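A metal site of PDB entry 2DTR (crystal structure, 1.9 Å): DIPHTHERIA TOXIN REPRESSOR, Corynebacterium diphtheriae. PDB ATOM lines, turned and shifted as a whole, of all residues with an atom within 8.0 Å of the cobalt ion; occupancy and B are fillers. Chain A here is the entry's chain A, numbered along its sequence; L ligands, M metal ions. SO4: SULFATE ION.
ND1 of His 79 sits close to NH2 of Arg 13 (3.1 Å).
A ring nitrogen (ND1) of His 79 sits at hydrogen-bond distance from the backbone carbonyl oxygen of Ala 101, 3.3 Å away.
ND1 of His 79 is in hydrogen-bond range of OE1 of Glu 105 (2.8 Å).
Within 4 Å of the cobalt ion: His 79, Glu 83 and His 98.
The cobalt ion is bound by a ring nitrogen (ND1) of His 98 (2.0 Å), the side-chain carboxylate (OE2) of Glu 83 (2.0 Å), an oxygen (O4) of the ligand (2.1 Å) and a ring nitrogen (NE2) of His 79 (2.2 Å).
The cobalt ion has four donor atoms within binding distance.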
ATOM      1  N   ARG A  13      13.096  16.581 -14.891  1.00  0.00           N
ATOM      2  CA  ARG A  13      13.420  15.173 -15.065  1.00  0.00           C
ATOM      3  C   ARG A  13      14.951  14.968 -15.049  1.00  0.00           C
ATOM      4  O   ARG A  13      15.416  13.878 -14.681  1.00  0.00           O
ATOM      5  CB  ARG A  13      12.796  14.590 -16.338  1.00  0.00           C
ATOM      6  CG  ARG A  13      13.257  15.260 -17.623  1.00  0.00           C
ATOM      7  CD  ARG A  13      14.250  14.419 -18.414  1.00  0.00           C
ATOM      8  NE  ARG A  13      13.644  13.161 -18.848  1.00  0.00           N
ATOM      9  CZ  ARG A  13      14.236  11.981 -18.730  1.00  0.00           C
ATOM     10  NH1 ARG A  13      15.435  11.921 -18.185  1.00  0.00           N
ATOM     11  NH2 ARG A  13      13.618  10.875 -19.145  1.00  0.00           N
ATOM     12  N   GLU A  17      16.815  12.359 -12.700  1.00  0.00           N
ATOM     13  CA  GLU A  17      17.712  11.404 -13.285  1.00  0.00           C
ATOM     14  C   GLU A  17      19.077  11.333 -12.559  1.00  0.00           C
ATOM     15  O   GLU A  17      19.525  10.240 -12.158  1.00  0.00           O
ATOM     16  CB  GLU A  17      17.837  11.765 -14.764  1.00  0.00           C
ATOM     17  CG  GLU A  17      18.519  10.772 -15.632  1.00  0.00           C
ATOM     18  CD  GLU A  17      18.732  11.321 -17.014  1.00  0.00           C
ATOM     19  OE1 GLU A  17      18.913  12.539 -17.152  1.00  0.00           O
ATOM     20  OE2 GLU A  17      18.711  10.523 -17.964  1.00  0.00           O
ATOM     21  N   MET A  76       9.001  11.193 -15.579  1.00  0.00           N
ATOM     22  CA  MET A  76       9.812   9.978 -15.635  1.00  0.00           C
ATOM     23  C   MET A  76       8.967   8.729 -15.863  1.00  0.00           C
ATOM     24  O   MET A  76       9.404   7.797 -16.521  1.00  0.00           O
ATOM     25  CB  MET A  76      10.667   9.833 -14.377  1.00  0.00           C
ATOM     26  CG  MET A  76      11.765  10.926 -14.240  1.00  0.00           C
ATOM     27  CE  MET A  76      13.159   9.131 -15.768  1.00  0.00           C
ATOM     28  N   HIS A  79       7.978   8.817 -19.622  1.00  0.00           N
ATOM     29  CA  HIS A  79       9.173   8.460 -20.359  1.00  0.00           C
ATOM     30  C   HIS A  79       9.366   6.940 -20.413  1.00  0.00           C
ATOM     31  O   HIS A  79       9.505   6.359 -21.488  1.00  0.00           O
ATOM     32  CB  HIS A  79      10.367   9.130 -19.653  1.00  0.00           C
ATOM     33  CG  HIS A  79      11.700   8.796 -20.256  1.00  0.00           C
ATOM     34  ND1 HIS A  79      12.118   9.372 -21.425  1.00  0.00           N
ATOM     35  CD2 HIS A  79      12.595   7.861 -19.876  1.00  0.00           C
ATOM     36  CE1 HIS A  79      13.245   8.774 -21.736  1.00  0.00           C
ATOM     37  NE2 HIS A  79      13.582   7.860 -20.844  1.00  0.00           N
ATOM     38  N   ARG A  80       9.344   6.312 -19.245  1.00  0.00           N
ATOM     39  CA  ARG A  80       9.567   4.881 -19.140  1.00  0.00           C
ATOM     40  C   ARG A  80       8.430   3.963 -19.637  1.00  0.00           C
ATOM     41  O   ARG A  80       8.688   2.819 -20.071  1.00  0.00           O
ATOM     42  CB  ARG A  80      10.016   4.548 -17.700  1.00  0.00           C
ATOM     43  CG  ARG A  80      11.371   5.149 -17.406  1.00  0.00           C
ATOM     44  CD  ARG A  80      11.891   4.890 -15.982  1.00  0.00           C
ATOM     45  NE  ARG A  80      13.243   5.464 -15.887  1.00  0.00           N
ATOM     46  CZ  ARG A  80      13.893   5.762 -14.770  1.00  0.00           C
ATOM     47  NH1 ARG A  80      13.357   5.538 -13.564  1.00  0.00           N
ATOM     48  NH2 ARG A  80      15.076   6.354 -14.877  1.00  0.00           N
ATOM     49  N   GLU A  83       8.976   4.009 -23.320  1.00  0.00           N
ATOM     50  CA  GLU A  83      10.052   3.094 -23.709  1.00  0.00           C
ATOM     51  C   GLU A  83       9.579   1.653 -23.774  1.00  0.00           C
ATOM     52  O   GLU A  83       9.997   0.916 -24.654  1.00  0.00           O
ATOM     53  CB  GLU A  83      11.217   3.199 -22.739  1.00  0.00           C
ATOM     54  CG  GLU A  83      11.855   4.539 -22.817  1.00  0.00           C
ATOM     55  CD  GLU A  83      13.089   4.636 -21.967  1.00  0.00           C
ATOM     56  OE1 GLU A  83      13.093   4.067 -20.863  1.00  0.00           O
ATOM     57  OE2 GLU A  83      14.046   5.280 -22.402  1.00  0.00           O
ATOM     58  N   VAL A  97      15.268   3.919 -28.781  1.00  0.00           N
ATOM     59  CA  VAL A  97      14.178   4.009 -27.847  1.00  0.00           C
ATOM     60  C   VAL A  97      14.278   5.213 -26.903  1.00  0.00           C
ATOM     61  O   VAL A  97      13.360   6.007 -26.815  1.00  0.00           O
ATOM     62  CB  VAL A  97      14.030   2.652 -27.096  1.00  0.00           C
ATOM     63  CG1 VAL A  97      13.179   2.763 -25.850  1.00  0.00           C
ATOM     64  CG2 VAL A  97      13.370   1.662 -28.004  1.00  0.00           C
ATOM     65  N   HIS A  98      15.417   5.371 -26.245  1.00  0.00           N
ATOM     66  CA  HIS A  98      15.603   6.450 -25.300  1.00  0.00           C
ATOM     67  C   HIS A  98      15.370   7.859 -25.829  1.00  0.00           C
ATOM     68  O   HIS A  98      14.609   8.623 -25.243  1.00  0.00           O
ATOM     69  CB  HIS A  98      16.981   6.377 -24.681  1.00  0.00           C
ATOM     70  CG  HIS A  98      17.204   7.445 -23.654  1.00  0.00           C
ATOM     71  ND1 HIS A  98      16.622   7.384 -22.416  1.00  0.00           N
ATOM     72  CD2 HIS A  98      17.921   8.583 -23.757  1.00  0.00           C
ATOM     73  CE1 HIS A  98      17.000   8.484 -21.786  1.00  0.00           C
ATOM     74  NE2 HIS A  98      17.773   9.239 -22.536  1.00  0.00           N
ATOM     75  N   ASP A  99      16.028   8.224 -26.912  1.00  0.00           N
ATOM     76  CA  ASP A  99      15.821   9.541 -27.503  1.00  0.00           C
ATOM     77  C   ASP A  99      14.359   9.786 -27.955  1.00  0.00           C
ATOM     78  O   ASP A  99      13.828  10.914 -27.894  1.00  0.00           O
ATOM     79  CB  ASP A  99      16.774   9.742 -28.693  1.00  0.00           C
ATOM     80  CG  ASP A  99      18.257   9.827 -28.275  1.00  0.00           C
ATOM     81  OD1 ASP A  99      18.591  10.479 -27.235  1.00  0.00           O
ATOM     82  OD2 ASP A  99      19.088   9.243 -28.999  1.00  0.00           O
ATOM     83  N   GLU A 100      13.693   8.736 -28.460  1.00  0.00           N
ATOM     84  CA  GLU A 100      12.317   8.885 -28.869  1.00  0.00           C
ATOM     85  C   GLU A 100      11.460   9.200 -27.620  1.00  0.00           C
ATOM     86  O   GLU A 100      10.715  10.164 -27.580  1.00  0.00           O
ATOM     87  CB  GLU A 100      11.824   7.611 -29.526  1.00  0.00           C
ATOM     88  CG  GLU A 100      10.445   7.769 -30.173  1.00  0.00           C
ATOM     89  CD  GLU A 100      10.482   8.366 -31.576  1.00  0.00           C
ATOM     90  OE1 GLU A 100      11.506   8.184 -32.258  1.00  0.00           O
ATOM     91  OE2 GLU A 100       9.464   8.983 -32.011  1.00  0.00           O
ATOM     92  N   ALA A 101      11.631   8.412 -26.567  1.00  0.00           N
ATOM     93  CA  ALA A 101      10.879   8.614 -25.340  1.00  0.00           C
ATOM     94  C   ALA A 101      11.131   9.964 -24.691  1.00  0.00           C
ATOM     95  O   ALA A 101      10.301  10.438 -23.933  1.00  0.00           O
ATOM     96  CB  ALA A 101      11.196   7.526 -24.365  1.00  0.00           C
ATOM     97  N   CYS A 102      12.315  10.527 -24.927  1.00  0.00           N
ATOM     98  CA  CYS A 102      12.688  11.829 -24.380  1.00  0.00           C
ATOM     99  C   CYS A 102      11.762  12.899 -24.915  1.00  0.00           C
ATOM    100  O   CYS A 102      11.590  13.939 -24.293  1.00  0.00           O
ATOM    101  CB  CYS A 102      14.161  12.192 -24.716  1.00  0.00           C
ATOM    102  N   GLU A 105       7.634  11.891 -23.650  1.00  0.00           N
ATOM    103  CA  GLU A 105       7.351  12.141 -22.242  1.00  0.00           C
ATOM    104  C   GLU A 105       6.644  13.465 -22.010  1.00  0.00           C
ATOM    105  O   GLU A 105       5.972  13.675 -21.003  1.00  0.00           O
ATOM    106  CB  GLU A 105       8.642  12.069 -21.432  1.00  0.00           C
ATOM    107  CG  GLU A 105       9.614  13.166 -21.735  1.00  0.00           C
ATOM    108  CD  GLU A 105      10.912  13.028 -20.981  1.00  0.00           C
ATOM    109  OE1 GLU A 105      11.226  11.915 -20.509  1.00  0.00           O
ATOM    110  OE2 GLU A 105      11.619  14.044 -20.839  1.00  0.00           O
ATOM    111  N   SER A 126      12.059   0.021 -16.800  1.00  0.00           N
ATOM    112  CA  SER A 126      12.259   0.457 -18.176  1.00  0.00           C
ATOM    113  C   SER A 126      13.175  -0.580 -18.854  1.00  0.00           C
ATOM    114  O   SER A 126      13.844  -1.399 -18.166  1.00  0.00           O
ATOM    115  CB  SER A 126      12.961   1.795 -18.186  1.00  0.00           C
ATOM    116  OG  SER A 126      14.307   1.676 -17.787  1.00  0.00           O
ATOM    117  N   PRO A 127      13.261  -0.555 -20.203  1.00  0.00           N
ATOM    118  CA  PRO A 127      14.157  -1.552 -20.822  1.00  0.00           C
ATOM    119  C   PRO A 127      15.630  -1.360 -20.409  1.00  0.00           C
ATOM    120  O   PRO A 127      16.433  -2.277 -20.487  1.00  0.00           O
ATOM    121  CB  PRO A 127      13.921  -1.400 -22.334  1.00  0.00           C
ATOM    122  CG  PRO A 127      12.995  -0.227 -22.492  1.00  0.00           C
ATOM    123  CD  PRO A 127      12.307   0.013 -21.188  1.00  0.00           C
ATOM    124  N   PHE A 128      15.931  -0.198 -19.872  1.00  0.00           N
ATOM    125  CA  PHE A 128      17.274   0.119 -19.454  1.00  0.00           C
ATOM    126  C   PHE A 128      17.542  -0.199 -18.002  1.00  0.00           C
ATOM    127  O   PHE A 128      18.565   0.159 -17.453  1.00  0.00           O
ATOM    128  CB  PHE A 128      17.597   1.565 -19.850  1.00  0.00           C
ATOM    129  CG  PHE A 128      17.405   1.803 -21.309  1.00  0.00           C
ATOM    130  CD1 PHE A 128      18.166   1.076 -22.239  1.00  0.00           C
ATOM    131  CD2 PHE A 128      16.367   2.571 -21.781  1.00  0.00           C
ATOM    132  CE1 PHE A 128      17.873   1.120 -23.605  1.00  0.00           C
ATOM    133  CE2 PHE A 128      16.068   2.617 -23.155  1.00  0.00           C
ATOM    134  CZ  PHE A 128      16.820   1.897 -24.053  1.00  0.00           C
ATOM    135  N   ASN A 130      15.754   0.632 -15.058  1.00  0.00           N
ATOM    136  CA  ASN A 130      15.347   1.475 -13.954  1.00  0.00           C
ATOM    137  C   ASN A 130      13.888   1.312 -13.689  1.00  0.00           C
ATOM    138  O   ASN A 130      13.129   1.089 -14.622  1.00  0.00           O
ATOM    139  CB  ASN A 130      15.599   2.925 -14.278  1.00  0.00           C
ATOM    140  CG  ASN A 130      17.048   3.239 -14.367  1.00  0.00           C
ATOM    141  OD1 ASN A 130      17.808   3.024 -13.416  1.00  0.00           O
ATOM    142  ND2 ASN A 130      17.478   3.714 -15.519  1.00  0.00           N
HETATM  143  S   SO4 L   1      15.859   5.374 -18.491  1.00  0.00           S
HETATM  144  O1  SO4 L   1      16.991   5.262 -17.539  1.00  0.00           O
HETATM  145  O2  SO4 L   1      15.036   4.141 -18.451  1.00  0.00           O
HETATM  146  O3  SO4 L   1      15.017   6.528 -18.101  1.00  0.00           O
HETATM  147  O4  SO4 L   1      16.402   5.591 -19.886  1.00  0.00           O
HETATM  148 CO    CO M   1      15.210   6.526 -21.300  1.00  0.00          CO
